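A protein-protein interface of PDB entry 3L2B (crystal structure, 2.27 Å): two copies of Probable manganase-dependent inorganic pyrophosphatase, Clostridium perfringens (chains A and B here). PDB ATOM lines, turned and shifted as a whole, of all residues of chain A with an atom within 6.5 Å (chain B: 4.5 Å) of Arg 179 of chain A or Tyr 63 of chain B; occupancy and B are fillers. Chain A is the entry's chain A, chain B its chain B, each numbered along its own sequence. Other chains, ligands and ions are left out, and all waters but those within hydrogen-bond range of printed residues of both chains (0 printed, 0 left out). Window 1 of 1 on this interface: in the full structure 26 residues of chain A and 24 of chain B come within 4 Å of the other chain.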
ATOM      1  N   ILE A  59      15.287   1.685  -3.149  1.00  0.00           N
ATOM      2  CA  ILE A  59      14.436   2.058  -4.272  1.00  0.00           C
ATOM      3  C   ILE A  59      15.063   3.269  -4.967  1.00  0.00           C
ATOM      4  O   ILE A  59      15.224   3.280  -6.193  1.00  0.00           O
ATOM      5  CB  ILE A  59      13.001   2.459  -3.843  1.00  0.00           C
ATOM      6  CG1 ILE A  59      12.252   1.266  -3.185  1.00  0.00           C
ATOM      7  CG2 ILE A  59      12.198   2.979  -5.059  1.00  0.00           C
ATOM      8  CD1 ILE A  59      10.797   1.550  -2.807  1.00  0.00           C
ATOM      9  N   TYR A  63      16.326   3.439  -8.769  1.00  0.00           N
ATOM     10  CA  TYR A  63      15.713   4.391  -9.715  1.00  0.00           C
ATOM     11  C   TYR A  63      16.714   5.393 -10.243  1.00  0.00           C
ATOM     12  O   TYR A  63      16.701   5.728 -11.402  1.00  0.00           O
ATOM     13  CB  TYR A  63      14.544   5.162  -9.110  1.00  0.00           C
ATOM     14  CG  TYR A  63      13.367   4.289  -8.861  1.00  0.00           C
ATOM     15  CD1 TYR A  63      13.303   3.043  -9.461  1.00  0.00           C
ATOM     16  CD2 TYR A  63      12.314   4.709  -8.043  1.00  0.00           C
ATOM     17  CE1 TYR A  63      12.265   2.215  -9.251  1.00  0.00           C
ATOM     18  CZ  TYR A  63      11.245   2.628  -8.453  1.00  0.00           C
ATOM     19  OH  TYR A  63      10.222   1.744  -8.292  1.00  0.00           O
ATOM     20  N   MET A  64      17.593   5.855  -9.382  1.00  0.00           N
ATOM     21  CA  MET A  64      18.565   6.881  -9.784  1.00  0.00           C
ATOM     22  C   MET A  64      19.718   6.316 -10.613  1.00  0.00           C
ATOM     23  O   MET A  64      20.530   7.080 -11.156  1.00  0.00           O
ATOM     24  CB  MET A  64      19.167   7.590  -8.582  1.00  0.00           C
ATOM     25  CG  MET A  64      18.166   8.262  -7.649  1.00  0.00           C
ATOM     26  SD  MET A  64      17.587   9.881  -8.180  1.00  0.00           S
ATOM     27  CE  MET A  64      19.100  10.854  -8.333  1.00  0.00           C
ATOM     28  N   SER A 174       5.686   6.548 -24.942  1.00  0.00           N
ATOM     29  CA  SER A 174       7.015   5.945 -24.806  1.00  0.00           C
ATOM     30  C   SER A 174       7.852   6.588 -23.722  1.00  0.00           C
ATOM     31  O   SER A 174       8.605   5.883 -23.021  1.00  0.00           O
ATOM     32  CB  SER A 174       7.772   5.820 -26.143  1.00  0.00           C
ATOM     33  OG  SER A 174       7.786   7.013 -26.873  1.00  0.00           O
ATOM     34  N   PHE A 175       7.702   7.895 -23.531  1.00  0.00           N
ATOM     35  CA  PHE A 175       8.403   8.550 -22.447  1.00  0.00           C
ATOM     36  C   PHE A 175       7.956   7.937 -21.121  1.00  0.00           C
ATOM     37  O   PHE A 175       8.778   7.630 -20.240  1.00  0.00           O
ATOM     38  CB  PHE A 175       8.141  10.067 -22.428  1.00  0.00           C
ATOM     39  CG  PHE A 175       8.514  10.741 -21.129  1.00  0.00           C
ATOM     40  CD1 PHE A 175       9.839  10.938 -20.797  1.00  0.00           C
ATOM     41  CD2 PHE A 175       7.535  11.211 -20.270  1.00  0.00           C
ATOM     42  CE1 PHE A 175      10.202  11.572 -19.621  1.00  0.00           C
ATOM     43  CE2 PHE A 175       7.871  11.873 -19.085  1.00  0.00           C
ATOM     44  CZ  PHE A 175       9.205  12.043 -18.748  1.00  0.00           C
ATOM     45  N   THR A 176       6.641   7.789 -20.979  1.00  0.00           N
ATOM     46  CA  THR A 176       6.051   7.324 -19.725  1.00  0.00           C
ATOM     47  C   THR A 176       6.405   5.859 -19.473  1.00  0.00           C
ATOM     48  O   THR A 176       6.824   5.501 -18.397  1.00  0.00           O
ATOM     49  CB  THR A 176       4.527   7.546 -19.673  1.00  0.00           C
ATOM     50  OG1 THR A 176       4.241   8.928 -19.907  1.00  0.00           O
ATOM     51  CG2 THR A 176       3.971   7.192 -18.323  1.00  0.00           C
ATOM     52  N   ALA A 177       6.295   5.032 -20.493  1.00  0.00           N
ATOM     53  CA  ALA A 177       6.642   3.613 -20.376  1.00  0.00           C
ATOM     54  C   ALA A 177       8.117   3.453 -19.964  1.00  0.00           C
ATOM     55  O   ALA A 177       8.478   2.582 -19.156  1.00  0.00           O
ATOM     56  CB  ALA A 177       6.376   2.861 -21.722  1.00  0.00           C
ATOM     57  N   SER A 178       8.951   4.334 -20.497  1.00  0.00           N
ATOM     58  CA  SER A 178      10.391   4.281 -20.227  1.00  0.00           C
ATOM     59  C   SER A 178      10.650   4.617 -18.770  1.00  0.00           C
ATOM     60  O   SER A 178      11.467   3.995 -18.113  1.00  0.00           O
ATOM     61  CB  SER A 178      11.165   5.216 -21.134  1.00  0.00           C
ATOM     62  OG  SER A 178      11.008   4.849 -22.501  1.00  0.00           O
ATOM     63  N   ARG A 179       9.895   5.575 -18.284  1.00  0.00           N
ATOM     64  CA  ARG A 179      10.061   6.122 -16.943  1.00  0.00           C
ATOM     65  C   ARG A 179       9.508   5.166 -15.903  1.00  0.00           C
ATOM     66  O   ARG A 179      10.019   5.070 -14.785  1.00  0.00           O
ATOM     67  CB  ARG A 179       9.376   7.516 -16.889  1.00  0.00           C
ATOM     68  CG  ARG A 179       9.403   8.246 -15.599  1.00  0.00           C
ATOM     69  CD  ARG A 179       8.650   9.583 -15.715  1.00  0.00           C
ATOM     70  NE  ARG A 179       7.188   9.478 -15.901  1.00  0.00           N
ATOM     71  CZ  ARG A 179       6.323   9.014 -14.985  1.00  0.00           C
ATOM     72  NH1 ARG A 179       6.741   8.565 -13.813  1.00  0.00           N
ATOM     73  NH2 ARG A 179       5.023   8.976 -15.254  1.00  0.00           N
ATOM     74  N   LEU A 180       8.497   4.408 -16.309  1.00  0.00           N
ATOM     75  CA  LEU A 180       7.785   3.502 -15.400  1.00  0.00           C
ATOM     76  C   LEU A 180       8.340   2.094 -15.321  1.00  0.00           C
ATOM     77  O   LEU A 180       8.150   1.401 -14.331  1.00  0.00           O
ATOM     78  CB  LEU A 180       6.333   3.345 -15.840  1.00  0.00           C
ATOM     79  CG  LEU A 180       5.381   4.510 -15.669  1.00  0.00           C
ATOM     80  CD1 LEU A 180       4.083   4.228 -16.477  1.00  0.00           C
ATOM     81  CD2 LEU A 180       5.064   4.732 -14.178  1.00  0.00           C
ATOM     82  N   ILE A 181       8.992   1.653 -16.386  1.00  0.00           N
ATOM     83  CA  ILE A 181       9.299   0.242 -16.527  1.00  0.00           C
ATOM     84  C   ILE A 181      10.245  -0.273 -15.431  1.00  0.00           C
ATOM     85  O   ILE A 181      10.165  -1.473 -15.057  1.00  0.00           O
ATOM     86  CB  ILE A 181       9.841  -0.104 -17.931  1.00  0.00           C
ATOM     87  CG1 ILE A 181       9.642  -1.599 -18.181  1.00  0.00           C
ATOM     88  CG2 ILE A 181      11.290   0.343 -18.034  1.00  0.00           C
ATOM     89  CD1 ILE A 181      10.097  -2.090 -19.539  1.00  0.00           C
ATOM     90  N   VAL A 182      11.086   0.599 -14.856  1.00  0.00           N
ATOM     91  CA  VAL A 182      12.012   0.134 -13.782  1.00  0.00           C
ATOM     92  C   VAL A 182      11.281  -0.157 -12.459  1.00  0.00           C
ATOM     93  O   VAL A 182      11.806  -0.845 -11.579  1.00  0.00           O
ATOM     94  CB  VAL A 182      13.168   1.064 -13.511  1.00  0.00           C
ATOM     95  CG1 VAL A 182      13.994   1.207 -14.808  1.00  0.00           C
ATOM     96  CG2 VAL A 182      12.680   2.442 -12.987  1.00  0.00           C
ATOM     97  N   GLN A 183      10.047   0.307 -12.373  1.00  0.00           N
ATOM     98  CA  GLN A 183       9.227   0.070 -11.198  1.00  0.00           C
ATOM     99  C   GLN A 183       8.692  -1.367 -11.191  1.00  0.00           C
ATOM    100  O   GLN A 183       8.029  -1.799 -10.275  1.00  0.00           O
ATOM    101  CB  GLN A 183       8.055   1.054 -11.175  1.00  0.00           C
ATOM    102  CG  GLN A 183       8.509   2.537 -11.252  1.00  0.00           C
ATOM    103  CD  GLN A 183       7.358   3.479 -11.016  1.00  0.00           C
ATOM    104  OE1 GLN A 183       6.275   3.042 -10.654  1.00  0.00           O
ATOM    105  NE2 GLN A 183       7.579   4.778 -11.232  1.00  0.00           N
ATOM    106  N   ILE B  59      12.335  11.631  -2.483  1.00  0.00           N
ATOM    107  CA  ILE B  59      12.785  11.296  -3.850  1.00  0.00           C
ATOM    108  C   ILE B  59      11.941  10.138  -4.436  1.00  0.00           C
ATOM    109  O   ILE B  59      11.485  10.193  -5.584  1.00  0.00           O
ATOM    110  CB  ILE B  59      14.284  10.945  -3.887  1.00  0.00           C
ATOM    111  CG1 ILE B  59      15.119  12.164  -3.505  1.00  0.00           C
ATOM    112  CG2 ILE B  59      14.713  10.437  -5.287  1.00  0.00           C
ATOM    113  CD1 ILE B  59      16.571  11.812  -3.171  1.00  0.00           C
ATOM    114  N   THR B  60      11.693   9.120  -3.614  1.00  0.00           N
ATOM    115  CA  THR B  60      10.929   7.939  -4.045  1.00  0.00           C
ATOM    116  C   THR B  60       9.499   8.317  -4.300  1.00  0.00           C
ATOM    117  O   THR B  60       8.901   7.898  -5.288  1.00  0.00           O
ATOM    118  CB  THR B  60      10.990   6.817  -2.997  1.00  0.00           C
ATOM    119  OG1 THR B  60      12.323   6.318  -2.944  1.00  0.00           O
ATOM    120  CG2 THR B  60      10.036   5.682  -3.308  1.00  0.00           C
ATOM    121  N   ALA B  61       8.946   9.138  -3.426  1.00  0.00           N
ATOM    122  CA  ALA B  61       7.551   9.564  -3.592  1.00  0.00           C
ATOM    123  C   ALA B  61       7.397  10.325  -4.899  1.00  0.00           C
ATOM    124  O   ALA B  61       6.388  10.221  -5.587  1.00  0.00           O
ATOM    125  CB  ALA B  61       7.066  10.404  -2.397  1.00  0.00           C
ATOM    126  N   THR B  62       8.424  11.061  -5.270  1.00  0.00           N
ATOM    127  CA  THR B  62       8.360  11.847  -6.493  1.00  0.00           C
ATOM    128  C   THR B  62       8.375  10.923  -7.685  1.00  0.00           C
ATOM    129  O   THR B  62       7.557  11.060  -8.581  1.00  0.00           O
ATOM    130  CB  THR B  62       9.493  12.879  -6.561  1.00  0.00           C
ATOM    131  OG1 THR B  62       9.317  13.788  -5.481  1.00  0.00           O
ATOM    132  CG2 THR B  62       9.484  13.627  -7.876  1.00  0.00           C
ATOM    133  N   TYR B  63       9.248   9.928  -7.646  1.00  0.00           N
ATOM    134  CA  TYR B  63       9.371   8.940  -8.738  1.00  0.00           C
ATOM    135  C   TYR B  63       8.165   8.009  -8.867  1.00  0.00           C
ATOM    136  O   TYR B  63       7.782   7.627  -9.956  1.00  0.00           O
ATOM    137  CB  TYR B  63      10.609   8.060  -8.554  1.00  0.00           C
ATOM    138  CG  TYR B  63      11.030   7.345  -9.817  1.00  0.00           C
ATOM    139  CD1 TYR B  63      11.921   7.939 -10.692  1.00  0.00           C
ATOM    140  CD2 TYR B  63      10.532   6.072 -10.141  1.00  0.00           C
ATOM    141  CE1 TYR B  63      12.315   7.309 -11.848  1.00  0.00           C
ATOM    142  CE2 TYR B  63      10.918   5.432 -11.309  1.00  0.00           C
ATOM    143  CZ  TYR B  63      11.815   6.061 -12.161  1.00  0.00           C
ATOM    144  OH  TYR B  63      12.244   5.467 -13.329  1.00  0.00           O
ATOM    145  N   MET B  64       7.589   7.625  -7.734  1.00  0.00           N
ATOM    146  CA  MET B  64       6.518   6.597  -7.724  1.00  0.00           C
ATOM    147  C   MET B  64       5.125   7.172  -7.890  1.00  0.00           C
ATOM    148  O   MET B  64       4.230   6.489  -8.363  1.00  0.00           O
ATOM    149  CB  MET B  64       6.532   5.795  -6.433  1.00  0.00           C
ATOM    150  CG  MET B  64       7.824   5.065  -6.144  1.00  0.00           C
ATOM    151  SD  MET B  64       8.252   3.814  -7.357  1.00  0.00           S
ATOM    152  CE  MET B  64       6.716   2.897  -7.499  1.00  0.00           C
ATOM    153  N   ASP B  65       4.950   8.429  -7.506  1.00  0.00           N
ATOM    154  CA  ASP B  65       3.626   9.045  -7.480  1.00  0.00           C
ATOM    155  C   ASP B  65       3.313   9.806  -8.749  1.00  0.00           C
ATOM    156  O   ASP B  65       4.193  10.357  -9.390  1.00  0.00           O
ATOM    157  CB  ASP B  65       3.476   9.940  -6.251  1.00  0.00           C
ATOM    158  CG  ASP B  65       3.508   9.138  -4.959  1.00  0.00           C
ATOM    159  OD1 ASP B  65       3.213   7.914  -5.014  1.00  0.00           O
ATOM    160  OD2 ASP B  65       3.824   9.720  -3.897  1.00  0.00           O
ATOM    161  N   TRP B  67       2.789  11.388 -12.092  1.00  0.00           N
ATOM    162  CA  TRP B  67       3.625  12.390 -12.738  1.00  0.00           C
ATOM    163  C   TRP B  67       2.759  13.483 -13.327  1.00  0.00           C
ATOM    164  O   TRP B  67       1.949  13.258 -14.229  1.00  0.00           O
ATOM    165  CB  TRP B  67       4.428  11.734 -13.855  1.00  0.00           C
ATOM    166  CG  TRP B  67       5.649  12.446 -14.276  1.00  0.00           C
ATOM    167  CD1 TRP B  67       6.859  12.460 -13.630  1.00  0.00           C
ATOM    168  CD2 TRP B  67       5.832  13.191 -15.492  1.00  0.00           C
ATOM    169  NE1 TRP B  67       7.774  13.192 -14.357  1.00  0.00           N
ATOM    170  CE2 TRP B  67       7.167  13.651 -15.503  1.00  0.00           C
ATOM    171  CE3 TRP B  67       4.988  13.533 -16.565  1.00  0.00           C
ATOM    172  CZ2 TRP B  67       7.676  14.444 -16.543  1.00  0.00           C
ATOM    173  CZ3 TRP B  67       5.500  14.317 -17.602  1.00  0.00           C
ATOM    174  CH2 TRP B  67       6.825  14.766 -17.578  1.00  0.00           C
ATOM    175  N   VAL B 182      13.851  13.201 -15.248  1.00  0.00           N
ATOM    176  CA  VAL B 182      13.196  13.304 -13.923  1.00  0.00           C
ATOM    177  C   VAL B 182      14.172  13.743 -12.827  1.00  0.00           C
ATOM    178  O   VAL B 182      13.818  14.413 -11.867  1.00  0.00           O
ATOM    179  CB  VAL B 182      12.635  11.931 -13.467  1.00  0.00           C
ATOM    180  CG1 VAL B 182      11.680  12.140 -12.274  1.00  0.00           C
ATOM    181  CG2 VAL B 182      11.984  11.094 -14.687  1.00  0.00           C
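Tyr 63 of chain B touches its own counterpart, Tyr 63 of chain A.
Tyr 63 of chain A touches Met 64 of chain B, but with the chains exchanged Met 64 of chain A does not touch Tyr 63 of chain B (6.0 Å).
Val 182 of chain A touches Tyr 63 of chain B, but with the chains exchanged Tyr 63 of chain A does not touch Val 182 of chain B (7.7 Å).
4 positions are printed for both chains.
Of the 10 pairs that touch across the chains among the printed residues, 1 has its exchanged pair printed and touching as well.
Of the printed residues of chain B, Ile 59 of chain A touches Thr 60.
Printed residues of chain B within 4 Å of Arg 179 of chain A: Tyr 63 (2.7 Å), Trp 67 (3.1 Å) and Val 182 (3.8 Å).
Ile 181 of chain A touches none of the printed residues of chain B.
Of the printed residues of chain B, Val 182 of chain A touches Tyr 63.
Printed residues of chain B within 4 Å of Gln 183 of chain A: Tyr 63 (3.1 Å) and Met 64 (3.2 Å).
Ile 59 of chain B touches none of the printed residues of chain A.
Printed residues of chain A within 4 Å of Tyr 63 of chain B: Tyr 63 (3.1 Å), Arg 179 (2.7 Å), Val 182 (3.1 Å) and Gln 183 (3.1 Å).
Of the printed residues of chain A, Trp 67 of chain B touches Phe 175 (3.4 Å) and Arg 179 (3.1 Å).
The nearest printed residue of chain B that does not touch Arg 179 of chain A is Asp 65 of chain B (5.4 Å).
The nearest printed residue of chain A that does not touch Trp 67 of chain B is Thr 176 of chain A (5.7 Å).
Among the printed residues, pairs that only touch across the chains: Ile 59 of chain A with Thr 60 of chain B, Tyr 63 of chain A with Tyr 63 of chain B, Phe 175 of chain A with Trp 67 of chain B, Arg 179 of chain A with Trp 67 of chain B, Arg 179 of chain A with Val 182 of chain B, Val 182 of chain A with Tyr 63 of chain B and Gln 183 of chain A with Met 64 of chain B.
Of the 9 printed residues of chain B, 5 touch a printed residue of chain A.
Hydrophobic or aromatic side chains of chain B that line the printed part of chain A: Tyr 63, Met 64, Trp 67 and Val 182.
Among the printed residues, 10 pairs touch across the chains.
Among the printed residues, no Asp or Glu carboxylate lies within 4 Å of a Lys or Arg side-chain nitrogen of the other chain.
The side-chain hydroxyl (OH) of Tyr 63 of chain A lies within hydrogen-bond range of the side-chain sulfur (SD) of Met 64 of chain B, 3.0 Å away.
OH of Tyr 63 of chain B lies within hydrogen-bond range of O of Arg 179 of chain A (2.7 Å).
O of Tyr 63 of chain B is in hydrogen-bond range of NE2 of Gln 183 of chain A (3.1 Å).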
